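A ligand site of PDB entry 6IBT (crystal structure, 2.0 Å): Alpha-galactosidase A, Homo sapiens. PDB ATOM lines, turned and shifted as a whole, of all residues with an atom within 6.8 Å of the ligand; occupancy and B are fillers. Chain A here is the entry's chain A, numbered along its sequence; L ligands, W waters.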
ATOM      1  N   LEU A  14      -5.979  20.346  17.152  1.00  0.00           N
ATOM      2  CA  LEU A  14      -5.400  21.700  16.958  1.00  0.00           C
ATOM      3  C   LEU A  14      -5.361  21.983  15.444  1.00  0.00           C
ATOM      4  O   LEU A  14      -4.932  21.087  14.701  1.00  0.00           O
ATOM      5  CB  LEU A  14      -4.011  21.615  17.590  1.00  0.00           C
ATOM      6  CG  LEU A  14      -3.168  22.878  17.639  1.00  0.00           C
ATOM      7  CD1 LEU A  14      -3.883  23.989  18.387  1.00  0.00           C
ATOM      8  CD2 LEU A  14      -1.847  22.576  18.295  1.00  0.00           C
ATOM      9  N   TRP A  16      -3.554  23.922  13.417  1.00  0.00           N
ATOM     10  CA  TRP A  16      -2.422  24.597  12.710  1.00  0.00           C
ATOM     11  C   TRP A  16      -1.913  23.804  11.492  1.00  0.00           C
ATOM     12  O   TRP A  16      -1.889  24.355  10.397  1.00  0.00           O
ATOM     13  CB  TRP A  16      -1.237  24.865  13.624  1.00  0.00           C
ATOM     14  CG  TRP A  16      -0.208  25.680  12.917  1.00  0.00           C
ATOM     15  CD1 TRP A  16       1.058  25.314  12.555  1.00  0.00           C
ATOM     16  CD2 TRP A  16      -0.392  27.016  12.425  1.00  0.00           C
ATOM     17  NE1 TRP A  16       1.687  26.351  11.922  1.00  0.00           N
ATOM     18  CE2 TRP A  16       0.819  27.407  11.818  1.00  0.00           C
ATOM     19  CE3 TRP A  16      -1.455  27.922  12.441  1.00  0.00           C
ATOM     20  CZ2 TRP A  16       0.973  28.655  11.234  1.00  0.00           C
ATOM     21  CZ3 TRP A  16      -1.291  29.164  11.864  1.00  0.00           C
ATOM     22  CH2 TRP A  16      -0.089  29.529  11.288  1.00  0.00           C
ATOM     23  N   ASP A  61      -5.445  27.615  17.030  1.00  0.00           N
ATOM     24  CA  ASP A  61      -4.040  28.082  16.907  1.00  0.00           C
ATOM     25  C   ASP A  61      -4.089  29.522  16.420  1.00  0.00           C
ATOM     26  O   ASP A  61      -5.141  30.161  16.604  1.00  0.00           O
ATOM     27  CB  ASP A  61      -3.236  27.140  16.014  1.00  0.00           C
ATOM     28  CG  ASP A  61      -1.759  27.113  16.361  1.00  0.00           C
ATOM     29  OD1 ASP A  61      -1.042  27.969  15.821  1.00  0.00           O
ATOM     30  OD2 ASP A  61      -1.348  26.223  17.164  1.00  0.00           O
ATOM     31  N   ASP A  62      -2.997  30.018  15.836  1.00  0.00           N
ATOM     32  CA  ASP A  62      -2.858  31.419  15.366  1.00  0.00           C
ATOM     33  C   ASP A  62      -3.947  31.722  14.317  1.00  0.00           C
ATOM     34  O   ASP A  62      -4.564  30.756  13.791  1.00  0.00           O
ATOM     35  CB  ASP A  62      -1.440  31.632  14.825  1.00  0.00           C
ATOM     36  CG  ASP A  62      -0.962  33.072  14.824  1.00  0.00           C
ATOM     37  OD1 ASP A  62      -1.788  33.978  15.073  1.00  0.00           O
ATOM     38  OD2 ASP A  62       0.229  33.259  14.570  1.00  0.00           O
ATOM     39  N   CYS A  63      -4.213  33.017  14.088  1.00  0.00           N
ATOM     40  CA  CYS A  63      -5.068  33.611  13.033  1.00  0.00           C
ATOM     41  C   CYS A  63      -6.575  33.522  13.385  1.00  0.00           C
ATOM     42  O   CYS A  63      -7.370  33.427  12.463  1.00  0.00           O
ATOM     43  CB  CYS A  63      -4.761  32.997  11.665  1.00  0.00           C
ATOM     44  SG  CYS A  63      -2.998  33.114  11.225  1.00  0.00           S
ATOM     45  N   TYR A 103      -4.937  30.422  21.493  1.00  0.00           N
ATOM     46  CA  TYR A 103      -3.519  30.703  21.151  1.00  0.00           C
ATOM     47  C   TYR A 103      -3.249  32.195  21.395  1.00  0.00           C
ATOM     48  O   TYR A 103      -4.156  33.007  21.123  1.00  0.00           O
ATOM     49  CB  TYR A 103      -3.259  30.305  19.703  1.00  0.00           C
ATOM     50  CG  TYR A 103      -1.972  30.804  19.105  1.00  0.00           C
ATOM     51  CD1 TYR A 103      -1.848  32.110  18.675  1.00  0.00           C
ATOM     52  CD2 TYR A 103      -0.897  29.954  18.895  1.00  0.00           C
ATOM     53  CE1 TYR A 103      -0.670  32.577  18.121  1.00  0.00           C
ATOM     54  CE2 TYR A 103       0.279  30.394  18.309  1.00  0.00           C
ATOM     55  CZ  TYR A 103       0.406  31.717  17.940  1.00  0.00           C
ATOM     56  OH  TYR A 103       1.550  32.180  17.363  1.00  0.00           O
ATOM     57  N   ASP A 105       0.697  34.893  21.897  1.00  0.00           N
ATOM     58  CA  ASP A 105       2.182  34.968  21.734  1.00  0.00           C
ATOM     59  C   ASP A 105       2.761  35.849  22.851  1.00  0.00           C
ATOM     60  O   ASP A 105       2.095  36.801  23.302  1.00  0.00           O
ATOM     61  CB  ASP A 105       2.535  35.388  20.299  1.00  0.00           C
ATOM     62  CG  ASP A 105       4.013  35.278  19.933  1.00  0.00           C
ATOM     63  OD1 ASP A 105       4.832  36.087  20.456  1.00  0.00           O
ATOM     64  OD2 ASP A 105       4.336  34.406  19.103  1.00  0.00           O
ATOM     65  N   THR A 110       1.945  37.792  17.307  1.00  0.00           N
ATOM     66  CA  THR A 110       1.879  36.341  17.018  1.00  0.00           C
ATOM     67  C   THR A 110       2.772  36.089  15.802  1.00  0.00           C
ATOM     68  O   THR A 110       3.143  37.066  15.143  1.00  0.00           O
ATOM     69  CB  THR A 110       0.435  35.878  16.801  1.00  0.00           C
ATOM     70  OG1 THR A 110      -0.014  36.288  15.508  1.00  0.00           O
ATOM     71  CG2 THR A 110      -0.499  36.418  17.867  1.00  0.00           C
ATOM     72  N   CYS A 111       3.129  34.830  15.540  1.00  0.00           N
ATOM     73  CA  CYS A 111       4.063  34.502  14.434  1.00  0.00           C
ATOM     74  C   CYS A 111       3.434  34.919  13.101  1.00  0.00           C
ATOM     75  O   CYS A 111       4.168  35.446  12.262  1.00  0.00           O
ATOM     76  CB  CYS A 111       4.463  33.027  14.468  1.00  0.00           C
ATOM     77  SG  CYS A 111       5.231  32.542  16.033  1.00  0.00           S
ATOM     78  N   ALA A 112       2.118  34.798  12.945  1.00  0.00           N
ATOM     79  CA  ALA A 112       1.407  35.170  11.700  1.00  0.00           C
ATOM     80  C   ALA A 112       1.111  36.685  11.675  1.00  0.00           C
ATOM     81  O   ALA A 112       0.502  37.149  10.710  1.00  0.00           O
ATOM     82  CB  ALA A 112       0.141  34.343  11.546  1.00  0.00           C
ATOM     83  N   GLY A 113       1.497  37.422  12.715  1.00  0.00           N
ATOM     84  CA  GLY A 113       1.572  38.897  12.695  1.00  0.00           C
ATOM     85  C   GLY A 113       0.351  39.590  13.270  1.00  0.00           C
ATOM     86  O   GLY A 113       0.137  40.768  12.930  1.00  0.00           O
ATOM     87  N   LYS A 137      -2.181  27.920  24.341  1.00  0.00           N
ATOM     88  CA  LYS A 137      -0.893  27.689  23.663  1.00  0.00           C
ATOM     89  C   LYS A 137      -0.244  29.057  23.464  1.00  0.00           C
ATOM     90  O   LYS A 137      -0.875  29.917  22.844  1.00  0.00           O
ATOM     91  CB  LYS A 137      -1.125  26.989  22.312  1.00  0.00           C
ATOM     92  CG  LYS A 137       0.148  26.640  21.559  1.00  0.00           C
ATOM     93  CD  LYS A 137      -0.094  26.240  20.144  1.00  0.00           C
ATOM     94  CE  LYS A 137       1.192  26.130  19.339  1.00  0.00           C
ATOM     95  NZ  LYS A 137       0.983  25.343  18.112  1.00  0.00           N
ATOM     96  N   ASP A 139       2.905  30.945  21.989  1.00  0.00           N
ATOM     97  CA  ASP A 139       4.033  30.913  21.040  1.00  0.00           C
ATOM     98  C   ASP A 139       5.016  32.043  21.398  1.00  0.00           C
ATOM     99  O   ASP A 139       4.652  32.893  22.226  1.00  0.00           O
ATOM    100  CB  ASP A 139       3.479  30.984  19.619  1.00  0.00           C
ATOM    101  CG  ASP A 139       4.283  30.220  18.592  1.00  0.00           C
ATOM    102  OD1 ASP A 139       5.450  29.989  18.815  1.00  0.00           O
ATOM    103  OD2 ASP A 139       3.586  29.840  17.375  1.00  0.00           O
ATOM    104  N   GLY A 140       6.217  32.070  20.805  1.00  0.00           N
ATOM    105  CA  GLY A 140       7.330  32.896  21.272  1.00  0.00           C
ATOM    106  C   GLY A 140       7.912  33.827  20.222  1.00  0.00           C
ATOM    107  O   GLY A 140       9.053  34.262  20.446  1.00  0.00           O
ATOM    108  N   CYS A 141       7.199  34.132  19.139  1.00  0.00           N
ATOM    109  CA  CYS A 141       7.734  35.020  18.067  1.00  0.00           C
ATOM    110  C   CYS A 141       7.722  36.481  18.549  1.00  0.00           C
ATOM    111  O   CYS A 141       6.922  36.813  19.491  1.00  0.00           O
ATOM    112  CB  CYS A 141       6.940  34.912  16.764  1.00  0.00           C
ATOM    113  SG  CYS A 141       7.148  33.321  15.912  1.00  0.00           S
ATOM    114  N   GLU A 172       6.174  27.549  24.682  1.00  0.00           N
ATOM    115  CA  GLU A 172       7.217  27.314  23.659  1.00  0.00           C
ATOM    116  C   GLU A 172       8.539  27.918  24.127  1.00  0.00           C
ATOM    117  O   GLU A 172       9.442  28.093  23.292  1.00  0.00           O
ATOM    118  CB  GLU A 172       6.733  27.825  22.298  1.00  0.00           C
ATOM    119  CG  GLU A 172       5.426  27.167  21.884  1.00  0.00           C
ATOM    120  CD  GLU A 172       5.123  27.175  20.403  1.00  0.00           C
ATOM    121  OE1 GLU A 172       6.021  26.817  19.612  1.00  0.00           O
ATOM    122  OE2 GLU A 172       3.987  27.554  20.058  1.00  0.00           O
ATOM    123  N   LEU A 175      11.951  25.979  23.146  1.00  0.00           N
ATOM    124  CA  LEU A 175      12.178  26.119  21.684  1.00  0.00           C
ATOM    125  C   LEU A 175      12.827  27.475  21.371  1.00  0.00           C
ATOM    126  O   LEU A 175      13.800  27.491  20.604  1.00  0.00           O
ATOM    127  CB  LEU A 175      10.850  25.960  20.932  1.00  0.00           C
ATOM    128  CG  LEU A 175      10.910  26.316  19.448  1.00  0.00           C
ATOM    129  CD1 LEU A 175      11.942  25.434  18.742  1.00  0.00           C
ATOM    130  CD2 LEU A 175       9.532  26.201  18.813  1.00  0.00           C
ATOM    131  N   TYR A 176      12.300  28.584  21.901  1.00  0.00           N
ATOM    132  CA  TYR A 176      12.763  29.965  21.571  1.00  0.00           C
ATOM    133  C   TYR A 176      14.065  30.318  22.287  1.00  0.00           C
ATOM    134  O   TYR A 176      14.820  31.164  21.779  1.00  0.00           O
ATOM    135  CB  TYR A 176      11.629  30.985  21.774  1.00  0.00           C
ATOM    136  CG  TYR A 176      10.707  30.914  20.595  1.00  0.00           C
ATOM    137  CD1 TYR A 176      10.968  31.637  19.433  1.00  0.00           C
ATOM    138  CD2 TYR A 176       9.661  30.014  20.571  1.00  0.00           C
ATOM    139  CE1 TYR A 176      10.141  31.533  18.323  1.00  0.00           C
ATOM    140  CE2 TYR A 176       8.820  29.898  19.484  1.00  0.00           C
ATOM    141  CZ  TYR A 176       9.072  30.654  18.347  1.00  0.00           C
ATOM    142  OH  TYR A 176       8.239  30.500  17.297  1.00  0.00           O
ATOM    143  N   ARG A 196       7.054  23.079  24.116  1.00  0.00           N
ATOM    144  CA  ARG A 196       7.609  22.739  22.789  1.00  0.00           C
ATOM    145  C   ARG A 196       9.144  22.841  22.883  1.00  0.00           C
ATOM    146  O   ARG A 196       9.668  23.875  23.352  1.00  0.00           O
ATOM    147  CB  ARG A 196       6.956  23.617  21.712  1.00  0.00           C
ATOM    148  CG  ARG A 196       5.544  23.176  21.324  1.00  0.00           C
ATOM    149  CD  ARG A 196       5.546  22.041  20.297  1.00  0.00           C
ATOM    150  NE  ARG A 196       6.439  22.354  19.204  1.00  0.00           N
ATOM    151  CZ  ARG A 196       6.195  23.275  18.252  1.00  0.00           C
ATOM    152  NH1 ARG A 196       5.042  23.947  18.203  1.00  0.00           N
ATOM    153  NH2 ARG A 196       7.137  23.528  17.360  1.00  0.00           N
ATOM    154  N   PHE A 198      11.150  21.783  19.950  1.00  0.00           N
ATOM    155  CA  PHE A 198      11.731  21.639  18.586  1.00  0.00           C
ATOM    156  C   PHE A 198      10.857  22.329  17.540  1.00  0.00           C
ATOM    157  O   PHE A 198       9.678  22.664  17.798  1.00  0.00           O
ATOM    158  CB  PHE A 198      11.988  20.164  18.273  1.00  0.00           C
ATOM    159  CG  PHE A 198      12.925  19.914  17.120  1.00  0.00           C
ATOM    160  CD1 PHE A 198      14.263  20.277  17.202  1.00  0.00           C
ATOM    161  CD2 PHE A 198      12.470  19.352  15.930  1.00  0.00           C
ATOM    162  CE1 PHE A 198      15.134  20.056  16.147  1.00  0.00           C
ATOM    163  CE2 PHE A 198      13.340  19.154  14.857  1.00  0.00           C
ATOM    164  CZ  PHE A 198      14.666  19.504  14.971  1.00  0.00           C
ATOM    165  N   ALA A 199      11.447  22.559  16.369  1.00  0.00           N
ATOM    166  CA  ALA A 199      10.863  23.236  15.183  1.00  0.00           C
ATOM    167  C   ALA A 199       9.479  22.651  14.853  1.00  0.00           C
ATOM    168  O   ALA A 199       9.254  21.452  15.087  1.00  0.00           O
ATOM    169  CB  ALA A 199      11.813  23.120  14.013  1.00  0.00           C
ATOM    170  N   ASP A 200       8.589  23.502  14.354  1.00  0.00           N
ATOM    171  CA  ASP A 200       7.221  23.134  13.898  1.00  0.00           C
ATOM    172  C   ASP A 200       7.286  21.896  12.995  1.00  0.00           C
ATOM    173  O   ASP A 200       8.180  21.785  12.115  1.00  0.00           O
ATOM    174  CB  ASP A 200       6.553  24.269  13.126  1.00  0.00           C
ATOM    175  CG  ASP A 200       6.404  25.551  13.928  1.00  0.00           C
ATOM    176  OD1 ASP A 200       6.722  25.544  15.139  1.00  0.00           O
ATOM    177  OD2 ASP A 200       5.965  26.539  13.322  1.00  0.00           O
ATOM    178  N   ILE A 201       6.390  20.952  13.273  1.00  0.00           N
ATOM    179  CA  ILE A 201       6.236  19.714  12.482  1.00  0.00           C
ATOM    180  C   ILE A 201       5.641  20.091  11.097  1.00  0.00           C
ATOM    181  O   ILE A 201       4.879  21.092  11.018  1.00  0.00           O
ATOM    182  CB  ILE A 201       5.392  18.702  13.269  1.00  0.00           C
ATOM    183  CG1 ILE A 201       5.570  17.311  12.670  1.00  0.00           C
ATOM    184  CG2 ILE A 201       3.931  19.141  13.320  1.00  0.00           C
ATOM    185  CD1 ILE A 201       4.966  16.203  13.489  1.00  0.00           C
ATOM    186  N   ASP A 235       5.218  18.214  19.273  1.00  0.00           N
ATOM    187  CA  ASP A 235       4.290  18.802  18.284  1.00  0.00           C
ATOM    188  C   ASP A 235       3.213  17.776  17.860  1.00  0.00           C
ATOM    189  O   ASP A 235       3.195  16.634  18.358  1.00  0.00           O
ATOM    190  CB  ASP A 235       5.064  19.426  17.113  1.00  0.00           C
ATOM    191  CG  ASP A 235       4.411  20.694  16.571  1.00  0.00           C
ATOM    192  OD1 ASP A 235       3.279  20.991  17.011  1.00  0.00           O
ATOM    193  OD2 ASP A 235       5.008  21.357  15.709  1.00  0.00           O
ATOM    194  N   MET A 236       2.368  18.194  16.926  1.00  0.00           N
ATOM    195  CA  MET A 236       1.074  17.557  16.552  1.00  0.00           C
ATOM    196  C   MET A 236       1.272  16.193  15.868  1.00  0.00           C
ATOM    197  O   MET A 236       2.317  15.940  15.173  1.00  0.00           O
ATOM    198  CB  MET A 236       0.333  18.507  15.613  1.00  0.00           C
ATOM    199  CG  MET A 236      -0.030  19.857  16.272  1.00  0.00           C
ATOM    200  SD  MET A 236      -0.493  21.151  15.072  1.00  0.00           S
ATOM    201  CE  MET A 236       1.107  21.886  14.712  1.00  0.00           C
HETATM  202  C1  LIG L   1       3.933  29.423  15.095  1.00  0.00           C
HETATM  203  C2  LIG L   1       4.358  29.041  16.508  1.00  0.00           C
HETATM  204  C3  LIG L   1       4.152  27.549  16.824  1.00  0.00           C
HETATM  205  C4  LIG L   1       3.439  26.757  15.723  1.00  0.00           C
HETATM  206  C5  LIG L   1       2.209  27.529  15.317  1.00  0.00           C
HETATM  207  C6  LIG L   1       2.587  28.849  14.644  1.00  0.00           C
HETATM  208  O1  LIG L   1       1.423  27.696  16.504  1.00  0.00           O
HETATM  209  O2  LIG L   1       2.974  25.490  16.214  1.00  0.00           O
HETATM  210  O3  LIG L   1       5.427  26.947  17.054  1.00  0.00           O
HETATM  211  C7  LIG L   1       1.454  29.839  14.783  1.00  0.00           C
HETATM  212  O4  LIG L   1       1.727  31.056  14.077  1.00  0.00           O
HETATM  213  N1  LIG L   1       5.047  28.976  14.229  1.00  0.00           N
HETATM  214  O   HOH W   1       3.809  23.480  14.691  1.00  0.00           O
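Trp 16 touches the ligand. Cys 111 touches the ligand (CB to O4, 3.4 Å). Ala 112 touches the ligand. The nearest printed residue that does not touch the ligand is Tyr 176 (4.2 Å).
OD2 of Asp 139 sits at hydrogen-bond distance from OH of Tyr 103 (3.1 Å). The side-chain carboxylate (OD1) of Asp 139 is in hydrogen-bond range of the side-chain hydroxyl (OH) of Tyr 176 (3.2 Å). NZ of Lys 137 is in salt-bridge range of OD2 of Asp 61 (2.7 Å). The side-chain carboxylate (OE1) of Glu 172 is in salt-bridge range of the guanidinium group (NH1) of Arg 196 (3.3 Å). OD1 of Asp 200 is in salt-bridge range of NH2 of Arg 196 (3.0 Å). The side-chain carboxylate (OD2) of Asp 62 lies within hydrogen-bond range of the side-chain hydroxyl (OH) of Tyr 103 (3.3 Å). The side-chain hydroxyl (OG1) of Thr 110 sits at hydrogen-bond distance from the side-chain carboxylate (OD1) of Asp 62 (2.9 Å). N of Leu 175 is in hydrogen-bond range of O of Arg 196.
The side-chain carboxylate (OD2) of Asp 139 is covalently linked to a carbon (C2) of the ligand, 1.4 Å away. The side-chain carboxylate (OD1) of Asp 61 sits at hydrogen-bond distance from an oxygen (O1) of the ligand. The side-chain carboxylate (OE1) of Glu 172 lies within hydrogen-bond range of an oxygen (O3) of the ligand (2.6 Å). N1 of the ligand lies within salt-bridge range of OD2 of Asp 200, at 2.8 Å. The side-chain carboxylate (OD2) of Asp 62 lies within hydrogen-bond range of an oxygen (O4) of the ligand (2.7 Å). An oxygen (O2) of the ligand is in hydrogen-bond range of the side-chain amino group (NZ) of Lys 137 (2.8 Å). NH1 of Arg 196 lies within hydrogen-bond range of O3 of the ligand, 3.2 Å away. The side-chain hydroxyl (OH) of Tyr 103 lies within hydrogen-bond range of an oxygen (O4) of the ligand (3.5 Å).
Water W1 bridges OD2 of Asp 235 and O2 of the ligand.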
